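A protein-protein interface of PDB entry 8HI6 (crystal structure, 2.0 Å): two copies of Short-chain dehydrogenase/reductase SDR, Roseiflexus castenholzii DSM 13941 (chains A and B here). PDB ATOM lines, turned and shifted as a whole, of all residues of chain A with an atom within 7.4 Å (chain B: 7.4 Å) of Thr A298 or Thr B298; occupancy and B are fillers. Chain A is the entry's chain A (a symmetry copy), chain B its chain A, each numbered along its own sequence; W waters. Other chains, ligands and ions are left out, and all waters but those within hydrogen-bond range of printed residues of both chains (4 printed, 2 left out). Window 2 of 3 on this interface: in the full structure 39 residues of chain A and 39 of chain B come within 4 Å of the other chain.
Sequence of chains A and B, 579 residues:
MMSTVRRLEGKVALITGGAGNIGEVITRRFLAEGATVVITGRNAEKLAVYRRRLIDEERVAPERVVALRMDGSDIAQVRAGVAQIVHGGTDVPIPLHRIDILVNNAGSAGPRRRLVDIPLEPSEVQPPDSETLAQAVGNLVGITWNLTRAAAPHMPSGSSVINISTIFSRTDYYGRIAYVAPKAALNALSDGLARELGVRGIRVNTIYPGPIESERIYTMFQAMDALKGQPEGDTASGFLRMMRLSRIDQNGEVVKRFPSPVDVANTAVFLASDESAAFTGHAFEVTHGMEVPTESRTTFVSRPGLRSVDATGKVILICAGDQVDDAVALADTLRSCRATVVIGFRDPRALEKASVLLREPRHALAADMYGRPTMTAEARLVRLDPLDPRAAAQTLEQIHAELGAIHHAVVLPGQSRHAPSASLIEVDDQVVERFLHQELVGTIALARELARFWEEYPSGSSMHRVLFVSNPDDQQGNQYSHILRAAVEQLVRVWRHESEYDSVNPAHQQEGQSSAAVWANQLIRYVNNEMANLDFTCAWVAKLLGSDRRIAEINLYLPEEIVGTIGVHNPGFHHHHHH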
ATOM      1  N   GLU A 295      18.729  14.412   6.722  1.00  0.00           N
ATOM      2  CA  GLU A 295      18.986  14.490   5.288  1.00  0.00           C
ATOM      3  C   GLU A 295      19.306  15.924   4.891  1.00  0.00           C
ATOM      4  O   GLU A 295      18.689  16.863   5.396  1.00  0.00           O
ATOM      5  CB  GLU A 295      17.785  13.979   4.470  1.00  0.00           C
ATOM      6  CG  GLU A 295      18.107  13.804   2.966  1.00  0.00           C
ATOM      7  CD  GLU A 295      16.940  13.242   2.162  1.00  0.00           C
ATOM      8  OE1 GLU A 295      15.839  13.073   2.731  1.00  0.00           O
ATOM      9  OE2 GLU A 295      17.120  12.955   0.955  1.00  0.00           O
ATOM     10  N   SER A 296      20.264  16.088   3.975  1.00  0.00           N
ATOM     11  CA  SER A 296      20.513  17.372   3.322  1.00  0.00           C
ATOM     12  C   SER A 296      19.786  17.361   1.968  1.00  0.00           C
ATOM     13  O   SER A 296      20.202  16.654   1.037  1.00  0.00           O
ATOM     14  CB  SER A 296      22.019  17.597   3.156  1.00  0.00           C
ATOM     15  OG  SER A 296      22.287  18.723   2.336  1.00  0.00           O
ATOM     16  N   ARG A 297      18.700  18.127   1.852  1.00  0.00           N
ATOM     17  CA  ARG A 297      17.881  18.063   0.647  1.00  0.00           C
ATOM     18  C   ARG A 297      17.210  19.404   0.366  1.00  0.00           C
ATOM     19  O   ARG A 297      17.014  20.223   1.265  1.00  0.00           O
ATOM     20  CB  ARG A 297      16.816  16.953   0.753  1.00  0.00           C
ATOM     21  CG  ARG A 297      15.671  17.254   1.718  1.00  0.00           C
ATOM     22  CD  ARG A 297      14.451  16.337   1.443  1.00  0.00           C
ATOM     23  NE  ARG A 297      13.569  16.885   0.413  1.00  0.00           N
ATOM     24  CZ  ARG A 297      12.678  16.181  -0.278  1.00  0.00           C
ATOM     25  NH1 ARG A 297      12.482  14.890  -0.048  1.00  0.00           N
ATOM     26  NH2 ARG A 297      11.966  16.788  -1.227  1.00  0.00           N
ATOM     27  N   THR A 298      16.880  19.615  -0.910  1.00  0.00           N
ATOM     28  CA  THR A 298      16.013  20.698  -1.363  1.00  0.00           C
ATOM     29  C   THR A 298      15.214  20.165  -2.547  1.00  0.00           C
ATOM     30  O   THR A 298      15.532  19.115  -3.110  1.00  0.00           O
ATOM     31  CB  THR A 298      16.813  21.968  -1.750  1.00  0.00           C
ATOM     32  OG1 THR A 298      15.924  23.084  -1.940  1.00  0.00           O
ATOM     33  CG2 THR A 298      17.615  21.746  -3.038  1.00  0.00           C
ATOM     34  N   THR A 299      14.155  20.886  -2.912  1.00  0.00           N
ATOM     35  CA  THR A 299      13.272  20.492  -4.004  1.00  0.00           C
ATOM     36  C   THR A 299      13.307  21.558  -5.090  1.00  0.00           C
ATOM     37  O   THR A 299      13.171  22.745  -4.791  1.00  0.00           O
ATOM     38  CB  THR A 299      11.840  20.308  -3.499  1.00  0.00           C
ATOM     39  OG1 THR A 299      11.856  19.433  -2.365  1.00  0.00           O
ATOM     40  CG2 THR A 299      10.950  19.684  -4.583  1.00  0.00           C
ATOM     41  N   PHE A 300      13.463  21.140  -6.347  1.00  0.00           N
ATOM     42  CA  PHE A 300      13.408  22.098  -7.446  1.00  0.00           C
ATOM     43  C   PHE A 300      12.021  22.743  -7.503  1.00  0.00           C
ATOM     44  O   PHE A 300      11.007  22.049  -7.456  1.00  0.00           O
ATOM     45  CB  PHE A 300      13.711  21.403  -8.777  1.00  0.00           C
ATOM     46  CG  PHE A 300      15.131  20.915  -8.913  1.00  0.00           C
ATOM     47  CD1 PHE A 300      16.195  21.796  -8.855  1.00  0.00           C
ATOM     48  CD2 PHE A 300      15.393  19.573  -9.128  1.00  0.00           C
ATOM     49  CE1 PHE A 300      17.504  21.340  -9.003  1.00  0.00           C
ATOM     50  CE2 PHE A 300      16.698  19.112  -9.293  1.00  0.00           C
ATOM     51  CZ  PHE A 300      17.750  19.993  -9.226  1.00  0.00           C
ATOM     52  N   VAL A 301      11.969  24.074  -7.574  1.00  0.00           N
ATOM     53  CA  VAL A 301      10.683  24.755  -7.638  1.00  0.00           C
ATOM     54  C   VAL A 301      10.485  25.481  -8.962  1.00  0.00           C
ATOM     55  O   VAL A 301       9.498  26.196  -9.127  1.00  0.00           O
ATOM     56  CB  VAL A 301      10.498  25.719  -6.451  1.00  0.00           C
ATOM     57  CG1 VAL A 301      10.551  24.940  -5.137  1.00  0.00           C
ATOM     58  CG2 VAL A 301      11.546  26.805  -6.480  1.00  0.00           C
ATOM     59  N   ASN A 521      26.519  16.973  -6.046  1.00  0.00           N
ATOM     60  CA  ASN A 521      25.128  16.931  -5.627  1.00  0.00           C
ATOM     61  C   ASN A 521      24.562  15.618  -6.146  1.00  0.00           C
ATOM     62  O   ASN A 521      25.200  14.921  -6.939  1.00  0.00           O
ATOM     63  CB  ASN A 521      24.267  18.101  -6.177  1.00  0.00           C
ATOM     64  CG  ASN A 521      24.817  19.485  -5.826  1.00  0.00           C
ATOM     65  OD1 ASN A 521      25.630  20.043  -6.561  1.00  0.00           O
ATOM     66  ND2 ASN A 521      24.328  20.064  -4.735  1.00  0.00           N
ATOM     67  N   GLN A 522      23.341  15.296  -5.726  1.00  0.00           N
ATOM     68  CA  GLN A 522      22.656  14.094  -6.182  1.00  0.00           C
ATOM     69  C   GLN A 522      21.237  14.479  -6.594  1.00  0.00           C
ATOM     70  O   GLN A 522      20.492  15.031  -5.784  1.00  0.00           O
ATOM     71  CB  GLN A 522      22.640  13.031  -5.077  1.00  0.00           C
ATOM     72  CG  GLN A 522      21.746  11.842  -5.388  1.00  0.00           C
ATOM     73  CD  GLN A 522      21.860  10.702  -4.381  1.00  0.00           C
ATOM     74  OE1 GLN A 522      21.846   9.540  -4.772  1.00  0.00           O
ATOM     75  NE2 GLN A 522      21.935  11.029  -3.081  1.00  0.00           N
ATOM     76  N   ILE A 524      17.474  13.477  -7.517  1.00  0.00           N
ATOM     77  CA  ILE A 524      16.548  12.390  -7.237  1.00  0.00           C
ATOM     78  C   ILE A 524      15.376  12.485  -8.215  1.00  0.00           C
ATOM     79  O   ILE A 524      14.516  13.363  -8.091  1.00  0.00           O
ATOM     80  CB  ILE A 524      16.069  12.430  -5.781  1.00  0.00           C
ATOM     81  CG1 ILE A 524      17.282  12.369  -4.832  1.00  0.00           C
ATOM     82  CG2 ILE A 524      15.060  11.290  -5.509  1.00  0.00           C
ATOM     83  CD1 ILE A 524      18.056  11.072  -4.929  1.00  0.00           C
ATOM     84  N   ILE A 551      24.643  24.684  -5.557  1.00  0.00           N
ATOM     85  CA  ILE A 551      23.610  24.488  -4.543  1.00  0.00           C
ATOM     86  C   ILE A 551      24.226  23.812  -3.322  1.00  0.00           C
ATOM     87  O   ILE A 551      24.936  22.802  -3.446  1.00  0.00           O
ATOM     88  CB  ILE A 551      22.440  23.666  -5.104  1.00  0.00           C
ATOM     89  CG1 ILE A 551      21.774  24.426  -6.257  1.00  0.00           C
ATOM     90  CG2 ILE A 551      21.421  23.347  -4.004  1.00  0.00           C
ATOM     91  CD1 ILE A 551      20.831  23.556  -7.068  1.00  0.00           C
ATOM     92  N   ALA A 552      23.946  24.363  -2.140  1.00  0.00           N
ATOM     93  CA  ALA A 552      24.543  23.854  -0.907  1.00  0.00           C
ATOM     94  C   ALA A 552      23.971  22.492  -0.512  1.00  0.00           C
ATOM     95  O   ALA A 552      24.708  21.611  -0.055  1.00  0.00           O
ATOM     96  CB  ALA A 552      24.328  24.871   0.224  1.00  0.00           C
ATOM     97  N   GLU A 553      22.657  22.310  -0.638  1.00  0.00           N
ATOM     98  CA  GLU A 553      22.038  21.046  -0.266  1.00  0.00           C
ATOM     99  C   GLU A 553      22.551  19.920  -1.158  1.00  0.00           C
ATOM    100  O   GLU A 553      22.825  20.114  -2.346  1.00  0.00           O
ATOM    101  CB  GLU A 553      20.519  21.168  -0.391  1.00  0.00           C
ATOM    102  CG  GLU A 553      19.892  21.905   0.785  1.00  0.00           C
ATOM    103  CD  GLU A 553      19.956  23.423   0.632  1.00  0.00           C
ATOM    104  OE1 GLU A 553      19.689  24.126   1.636  1.00  0.00           O
ATOM    105  OE2 GLU A 553      20.317  23.918  -0.465  1.00  0.00           O
ATOM    106  N   ILE A 554      22.669  18.722  -0.578  1.00  0.00           N
ATOM    107  CA  ILE A 554      23.261  17.612  -1.322  1.00  0.00           C
ATOM    108  C   ILE A 554      22.245  16.986  -2.272  1.00  0.00           C
ATOM    109  O   ILE A 554      22.519  16.824  -3.470  1.00  0.00           O
ATOM    110  CB  ILE A 554      23.854  16.568  -0.356  1.00  0.00           C
ATOM    111  CG1 ILE A 554      25.046  17.175   0.399  1.00  0.00           C
ATOM    112  CG2 ILE A 554      24.333  15.345  -1.130  1.00  0.00           C
ATOM    113  CD1 ILE A 554      25.689  16.196   1.410  1.00  0.00           C
ATOM    114  N   ASN A 555      21.064  16.625  -1.761  1.00  0.00           N
ATOM    115  CA  ASN A 555      20.051  15.924  -2.547  1.00  0.00           C
ATOM    116  C   ASN A 555      19.062  16.921  -3.146  1.00  0.00           C
ATOM    117  O   ASN A 555      18.455  17.713  -2.422  1.00  0.00           O
ATOM    118  CB  ASN A 555      19.294  14.905  -1.695  1.00  0.00           C
ATOM    119  CG  ASN A 555      20.177  13.745  -1.236  1.00  0.00           C
ATOM    120  OD1 ASN A 555      21.259  13.506  -1.782  1.00  0.00           O
ATOM    121  ND2 ASN A 555      19.702  13.010  -0.244  1.00  0.00           N
ATOM    122  N   LEU A 556      18.884  16.853  -4.463  1.00  0.00           N
ATOM    123  CA  LEU A 556      18.049  17.792  -5.210  1.00  0.00           C
ATOM    124  C   LEU A 556      16.891  16.998  -5.786  1.00  0.00           C
ATOM    125  O   LEU A 556      17.076  16.231  -6.737  1.00  0.00           O
ATOM    126  CB  LEU A 556      18.852  18.479  -6.318  1.00  0.00           C
ATOM    127  CG  LEU A 556      20.262  18.943  -5.932  1.00  0.00           C
ATOM    128  CD1 LEU A 556      21.040  19.456  -7.157  1.00  0.00           C
ATOM    129  CD2 LEU A 556      20.163  20.041  -4.886  1.00  0.00           C
ATOM    130  N   TYR A 557      15.703  17.173  -5.210  1.00  0.00           N
ATOM    131  CA  TYR A 557      14.548  16.376  -5.587  1.00  0.00           C
ATOM    132  C   TYR A 557      13.760  17.050  -6.705  1.00  0.00           C
ATOM    133  O   TYR A 557      13.523  18.260  -6.672  1.00  0.00           O
ATOM    134  CB  TYR A 557      13.622  16.157  -4.382  1.00  0.00           C
ATOM    135  CG  TYR A 557      14.128  15.103  -3.411  1.00  0.00           C
ATOM    136  CD1 TYR A 557      15.152  15.389  -2.500  1.00  0.00           C
ATOM    137  CD2 TYR A 557      13.583  13.832  -3.405  1.00  0.00           C
ATOM    138  CE1 TYR A 557      15.619  14.419  -1.606  1.00  0.00           C
ATOM    139  CE2 TYR A 557      14.038  12.857  -2.520  1.00  0.00           C
ATOM    140  CZ  TYR A 557      15.048  13.152  -1.626  1.00  0.00           C
ATOM    141  OH  TYR A 557      15.468  12.169  -0.760  1.00  0.00           O
ATOM    142  N   LEU A 558      13.332  16.254  -7.680  1.00  0.00           N
ATOM    143  CA  LEU A 558      12.286  16.725  -8.576  1.00  0.00           C
ATOM    144  C   LEU A 558      11.008  16.949  -7.773  1.00  0.00           C
ATOM    145  O   LEU A 558      10.758  16.246  -6.794  1.00  0.00           O
ATOM    146  CB  LEU A 558      12.021  15.717  -9.690  1.00  0.00           C
ATOM    147  CG  LEU A 558      12.827  15.982 -10.971  1.00  0.00           C
ATOM    148  CD1 LEU A 558      14.310  15.809 -10.701  1.00  0.00           C
ATOM    149  CD2 LEU A 558      12.382  15.037 -12.082  1.00  0.00           C
ATOM    150  N   GLU B 295       9.801  18.129   9.192  1.00  0.00           N
ATOM    151  CA  GLU B 295       9.573  19.453   8.621  1.00  0.00           C
ATOM    152  C   GLU B 295       9.280  19.336   7.133  1.00  0.00           C
ATOM    153  O   GLU B 295       9.899  18.532   6.437  1.00  0.00           O
ATOM    154  CB  GLU B 295      10.782  20.380   8.844  1.00  0.00           C
ATOM    155  CG  GLU B 295      10.487  21.857   8.486  1.00  0.00           C
ATOM    156  CD  GLU B 295      11.662  22.789   8.759  1.00  0.00           C
ATOM    157  OE1 GLU B 295      12.749  22.298   9.134  1.00  0.00           O
ATOM    158  OE2 GLU B 295      11.501  24.023   8.610  1.00  0.00           O
ATOM    159  N   SER B 296       8.342  20.153   6.646  1.00  0.00           N
ATOM    160  CA  SER B 296       8.123  20.328   5.212  1.00  0.00           C
ATOM    161  C   SER B 296       8.875  21.593   4.770  1.00  0.00           C
ATOM    162  O   SER B 296       8.468  22.716   5.106  1.00  0.00           O
ATOM    163  CB  SER B 296       6.623  20.426   4.914  1.00  0.00           C
ATOM    164  OG  SER B 296       6.386  20.813   3.569  1.00  0.00           O
ATOM    165  N   ARG B 297       9.973  21.424   4.032  1.00  0.00           N
ATOM    166  CA  ARG B 297      10.815  22.566   3.694  1.00  0.00           C
ATOM    167  C   ARG B 297      11.509  22.361   2.352  1.00  0.00           C
ATOM    168  O   ARG B 297      11.698  21.232   1.894  1.00  0.00           O
ATOM    169  CB  ARG B 297      11.862  22.834   4.793  1.00  0.00           C
ATOM    170  CG  ARG B 297      12.992  21.809   4.864  1.00  0.00           C
ATOM    171  CD  ARG B 297      14.205  22.366   5.653  1.00  0.00           C
ATOM    172  NE  ARG B 297      15.114  23.134   4.802  1.00  0.00           N
ATOM    173  CZ  ARG B 297      16.008  24.013   5.242  1.00  0.00           C
ATOM    174  NH1 ARG B 297      16.183  24.238   6.538  1.00  0.00           N
ATOM    175  NH2 ARG B 297      16.746  24.685   4.360  1.00  0.00           N
ATOM    176  N   THR B 298      11.866  23.482   1.721  1.00  0.00           N
ATOM    177  CA  THR B 298      12.756  23.523   0.565  1.00  0.00           C
ATOM    178  C   THR B 298      13.569  24.807   0.674  1.00  0.00           C
ATOM    179  O   THR B 298      13.248  25.701   1.461  1.00  0.00           O
ATOM    180  CB  THR B 298      11.980  23.460  -0.776  1.00  0.00           C
ATOM    181  OG1 THR B 298      12.888  23.243  -1.873  1.00  0.00           O
ATOM    182  CG2 THR B 298      11.200  24.756  -1.025  1.00  0.00           C
ATOM    183  N   THR B 299      14.645  24.889  -0.109  1.00  0.00           N
ATOM    184  CA  THR B 299      15.544  26.037  -0.097  1.00  0.00           C
ATOM    185  C   THR B 299      15.543  26.690  -1.472  1.00  0.00           C
ATOM    186  O   THR B 299      15.689  26.000  -2.480  1.00  0.00           O
ATOM    187  CB  THR B 299      16.963  25.606   0.277  1.00  0.00           C
ATOM    188  OG1 THR B 299      16.913  24.843   1.488  1.00  0.00           O
ATOM    189  CG2 THR B 299      17.865  26.827   0.507  1.00  0.00           C
ATOM    190  N   PHE B 300      15.406  28.016  -1.514  1.00  0.00           N
ATOM    191  CA  PHE B 300      15.495  28.719  -2.791  1.00  0.00           C
ATOM    192  C   PHE B 300      16.891  28.531  -3.389  1.00  0.00           C
ATOM    193  O   PHE B 300      17.895  28.712  -2.702  1.00  0.00           O
ATOM    194  CB  PHE B 300      15.208  30.211  -2.600  1.00  0.00           C
ATOM    195  CG  PHE B 300      13.785  30.526  -2.216  1.00  0.00           C
ATOM    196  CD1 PHE B 300      12.731  30.183  -3.044  1.00  0.00           C
ATOM    197  CD2 PHE B 300      13.508  31.192  -1.035  1.00  0.00           C
ATOM    198  CE1 PHE B 300      11.419  30.496  -2.691  1.00  0.00           C
ATOM    199  CE2 PHE B 300      12.201  31.523  -0.683  1.00  0.00           C
ATOM    200  CZ  PHE B 300      11.160  31.171  -1.509  1.00  0.00           C
ATOM    201  N   VAL B 301      16.962  28.140  -4.662  1.00  0.00           N
ATOM    202  CA  VAL B 301      18.258  27.948  -5.299  1.00  0.00           C
ATOM    203  C   VAL B 301      18.491  28.939  -6.431  1.00  0.00           C
ATOM    204  O   VAL B 301      19.491  28.835  -7.140  1.00  0.00           O
ATOM    205  CB  VAL B 301      18.433  26.499  -5.792  1.00  0.00           C
ATOM    206  CG1 VAL B 301      18.345  25.535  -4.610  1.00  0.00           C
ATOM    207  CG2 VAL B 301      17.401  26.168  -6.843  1.00  0.00           C
ATOM    208  N   ASN B 521       2.292  29.341   2.252  1.00  0.00           N
ATOM    209  CA  ASN B 521       3.674  28.944   2.462  1.00  0.00           C
ATOM    210  C   ASN B 521       4.232  29.875   3.527  1.00  0.00           C
ATOM    211  O   ASN B 521       3.600  30.868   3.898  1.00  0.00           O
ATOM    212  CB  ASN B 521       4.561  29.047   1.191  1.00  0.00           C
ATOM    213  CG  ASN B 521       4.022  28.248   0.002  1.00  0.00           C
ATOM    214  OD1 ASN B 521       3.231  28.757  -0.790  1.00  0.00           O
ATOM    215  ND2 ASN B 521       4.499  27.018  -0.157  1.00  0.00           N
ATOM    216  N   GLN B 522       5.440  29.575   3.998  1.00  0.00           N
ATOM    217  CA  GLN B 522       6.118  30.407   4.983  1.00  0.00           C
ATOM    218  C   GLN B 522       7.550  30.642   4.507  1.00  0.00           C
ATOM    219  O   GLN B 522       8.286  29.683   4.281  1.00  0.00           O
ATOM    220  CB  GLN B 522       6.098  29.736   6.361  1.00  0.00           C
ATOM    221  CG  GLN B 522       6.982  30.423   7.387  1.00  0.00           C
ATOM    222  CD  GLN B 522       6.834  29.871   8.802  1.00  0.00           C
ATOM    223  OE1 GLN B 522       6.840  30.638   9.759  1.00  0.00           O
ATOM    224  NE2 GLN B 522       6.739  28.540   8.940  1.00  0.00           N
ATOM    225  N   ILE B 524      11.315  31.804   5.202  1.00  0.00           N
ATOM    226  CA  ILE B 524      12.222  31.902   6.337  1.00  0.00           C
ATOM    227  C   ILE B 524      13.414  32.772   5.934  1.00  0.00           C
ATOM    228  O   ILE B 524      14.283  32.342   5.169  1.00  0.00           O
ATOM    229  CB  ILE B 524      12.673  30.515   6.809  1.00  0.00           C
ATOM    230  CG1 ILE B 524      11.441  29.660   7.169  1.00  0.00           C
ATOM    231  CG2 ILE B 524      13.662  30.638   7.992  1.00  0.00           C
ATOM    232  CD1 ILE B 524      10.653  30.207   8.339  1.00  0.00           C
ATOM    233  N   ILE B 551       4.261  26.206  -4.783  1.00  0.00           N
ATOM    234  CA  ILE B 551       5.272  25.306  -4.232  1.00  0.00           C
ATOM    235  C   ILE B 551       4.623  24.402  -3.189  1.00  0.00           C
ATOM    236  O   ILE B 551       3.903  24.874  -2.297  1.00  0.00           O
ATOM    237  CB  ILE B 551       6.441  26.101  -3.631  1.00  0.00           C
ATOM    238  CG1 ILE B 551       7.139  26.913  -4.728  1.00  0.00           C
ATOM    239  CG2 ILE B 551       7.435  25.164  -2.934  1.00  0.00           C
ATOM    240  CD1 ILE B 551       8.086  27.962  -4.172  1.00  0.00           C
ATOM    241  N   ALA B 552       4.888  23.099  -3.295  1.00  0.00           N
ATOM    242  CA  ALA B 552       4.262  22.124  -2.405  1.00  0.00           C
ATOM    243  C   ALA B 552       4.807  22.214  -0.980  1.00  0.00           C
ATOM    244  O   ALA B 552       4.050  22.097  -0.010  1.00  0.00           O
ATOM    245  CB  ALA B 552       4.468  20.709  -2.967  1.00  0.00           C
ATOM    246  N   GLU B 553       6.120  22.376  -0.827  1.00  0.00           N
ATOM    247  CA  GLU B 553       6.716  22.454   0.499  1.00  0.00           C
ATOM    248  C   GLU B 553       6.204  23.685   1.240  1.00  0.00           C
ATOM    249  O   GLU B 553       5.957  24.738   0.645  1.00  0.00           O
ATOM    250  CB  GLU B 553       8.238  22.509   0.371  1.00  0.00           C
ATOM    251  CG  GLU B 553       8.853  21.143   0.095  1.00  0.00           C
ATOM    252  CD  GLU B 553       8.811  20.765  -1.384  1.00  0.00           C
ATOM    253  OE1 GLU B 553       9.069  19.577  -1.693  1.00  0.00           O
ATOM    254  OE2 GLU B 553       8.479  21.630  -2.233  1.00  0.00           O
ATOM    255  N   ILE B 554       6.059  23.555   2.562  1.00  0.00           N
ATOM    256  CA  ILE B 554       5.467  24.642   3.338  1.00  0.00           C
ATOM    257  C   ILE B 554       6.493  25.736   3.618  1.00  0.00           C
ATOM    258  O   ILE B 554       6.240  26.920   3.354  1.00  0.00           O
ATOM    259  CB  ILE B 554       4.842  24.102   4.638  1.00  0.00           C
ATOM    260  CG1 ILE B 554       3.644  23.200   4.306  1.00  0.00           C
ATOM    261  CG2 ILE B 554       4.362  25.255   5.512  1.00  0.00           C
ATOM    262  CD1 ILE B 554       2.969  22.597   5.560  1.00  0.00           C
ATOM    263  N   ASN B 555       7.659  25.364   4.156  1.00  0.00           N
ATOM    264  CA  ASN B 555       8.677  26.330   4.563  1.00  0.00           C
ATOM    265  C   ASN B 555       9.690  26.536   3.440  1.00  0.00           C
ATOM    266  O   ASN B 555      10.294  25.576   2.956  1.00  0.00           O
ATOM    267  CB  ASN B 555       9.405  25.870   5.827  1.00  0.00           C
ATOM    268  CG  ASN B 555       8.497  25.850   7.056  1.00  0.00           C
ATOM    269  OD1 ASN B 555       7.423  26.459   7.073  1.00  0.00           O
ATOM    270  ND2 ASN B 555       8.943  25.165   8.097  1.00  0.00           N
ATOM    271  N   LEU B 556       9.893  27.794   3.054  1.00  0.00           N
ATOM    272  CA  LEU B 556      10.754  28.161   1.933  1.00  0.00           C
ATOM    273  C   LEU B 556      11.913  28.960   2.502  1.00  0.00           C
ATOM    274  O   LEU B 556      11.736  30.119   2.892  1.00  0.00           O
ATOM    275  CB  LEU B 556       9.982  28.977   0.891  1.00  0.00           C
ATOM    276  CG  LEU B 556       8.572  28.473   0.562  1.00  0.00           C
ATOM    277  CD1 LEU B 556       7.824  29.457  -0.356  1.00  0.00           C
ATOM    278  CD2 LEU B 556       8.665  27.112  -0.108  1.00  0.00           C
ATOM    279  N   TYR B 557      13.091  28.342   2.558  1.00  0.00           N
ATOM    280  CA  TYR B 557      14.243  28.955   3.200  1.00  0.00           C
ATOM    281  C   TYR B 557      15.061  29.763   2.198  1.00  0.00           C
ATOM    282  O   TYR B 557      15.313  29.313   1.078  1.00  0.00           O
ATOM    283  CB  TYR B 557      15.143  27.887   3.837  1.00  0.00           C
ATOM    284  CG  TYR B 557      14.604  27.345   5.151  1.00  0.00           C
ATOM    285  CD1 TYR B 557      13.567  26.404   5.175  1.00  0.00           C
ATOM    286  CD2 TYR B 557      15.132  27.769   6.356  1.00  0.00           C
ATOM    287  CE1 TYR B 557      13.070  25.905   6.384  1.00  0.00           C
ATOM    288  CE2 TYR B 557      14.647  27.279   7.567  1.00  0.00           C
ATOM    289  CZ  TYR B 557      13.624  26.352   7.577  1.00  0.00           C
ATOM    290  OH  TYR B 557      13.175  25.882   8.790  1.00  0.00           O
ATOM    291  N   LEU B 558      15.497  30.947   2.618  1.00  0.00           N
ATOM    292  CA  LEU B 558      16.566  31.612   1.888  1.00  0.00           C
ATOM    293  C   LEU B 558      17.831  30.763   1.978  1.00  0.00           C
ATOM    294  O   LEU B 558      18.053  30.083   2.979  1.00  0.00           O
ATOM    295  CB  LEU B 558      16.839  33.000   2.456  1.00  0.00           C
ATOM    296  CG  LEU B 558      16.062  34.123   1.753  1.00  0.00           C
ATOM    297  CD1 LEU B 558      14.571  33.949   1.979  1.00  0.00           C
ATOM    298  CD2 LEU B 558      16.515  35.485   2.266  1.00  0.00           C
HETATM  299  O   HOH W   1      13.200  19.605  -0.026  1.00  0.00           O
HETATM  300  O   HOH W   2      15.528  22.606   2.105  1.00  0.00           O
HETATM  301  O   HOH W   3      20.124  26.448  -1.806  1.00  0.00           O
HETATM  302  O   HOH W   4       8.731  22.017  -5.065  1.00  0.00           O
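The side-chain hydroxyl (OG1) of Thr B298 sits at hydrogen-bond distance from the side-chain hydroxyl (OG1) of Thr A298 (3.0 Å). OG1 of Thr B298 lies within hydrogen-bond range of N of Thr A299, 2.9 Å away. N of Thr B299 lies within hydrogen-bond range of OG1 of Thr A298, 2.9 Å away. OG1 of Thr B299 is in hydrogen-bond range of OE1 of Glu A553 (2.9 Å). The side-chain carboxylate (OE1) of Glu B553 is in hydrogen-bond range of the side-chain hydroxyl (OG1) of Thr A299, 2.9 Å away.
N of Thr B298 lies within hydrogen-bond range of O of Asn B555 (2.9 Å). The guanidinium group of Arg A297 is in hydrogen-bond range of the side-chain hydroxyl of Thr A299 (2.9 Å). O of Asn A555 sits at hydrogen-bond distance from N of Thr A298 (2.9 Å).
Val A301 touches Ile B551 (CG1 to CG2, 3.8 Å). CG2 of Ile A551 touches CG1 of Val B301, at 3.8 Å.
Of chain B, only Thr B298 (3.0 Å) and Thr B299 (2.9 Å) come within 4 Å of Thr A298. Of chain A, only Thr A298 (3.0 Å) and Thr A299 (2.9 Å) come within 4 Å of Thr B298. Of the printed residues of chain A, Glu B553 touches Thr A299 (2.9 Å). Printed residues of chain A within 4 Å of Ile B551: Val A301 (3.8 Å). The nearest residue of chain A that does not touch Thr B298 is Val A301 (4.2 Å). The nearest printed residue of chain B that does not touch Val A301 is Thr B298 (4.2 Å).
Printed residues of chain A that touch a printed residue of chain B: Thr A298, Thr A299, Val A301, Ile A551 and Glu A553. Printed residues of chain B that touch a printed residue of chain A: Thr B298, Thr B299, Val B301, Ile B551 and Glu B553. Hydrophobic or aromatic side chains of chain B that line the printed part of chain A: Val B301 and Ile B551. Among the printed residues, 7 pairs touch across the chains. Among the printed residues, no Asp or Glu carboxylate lies within 4 Å of a Lys or Arg side-chain nitrogen of the other chain.
Thr B298 touches its own counterpart, Thr A298. Thr A298 touches Thr B299, and with the chains exchanged Thr A299 touches Thr B298. Thr A299 touches Glu B553, and with the chains exchanged Glu A553 touches Thr B299. Val A301 touches Ile B551, and with the chains exchanged Ile A551 touches Val B301.
Water W1 lies within hydrogen-bond range of OG1 of Thr A299 (2.7 Å), NE of Arg A297 (2.8 Å) and O of Arg B297 (2.9 Å).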
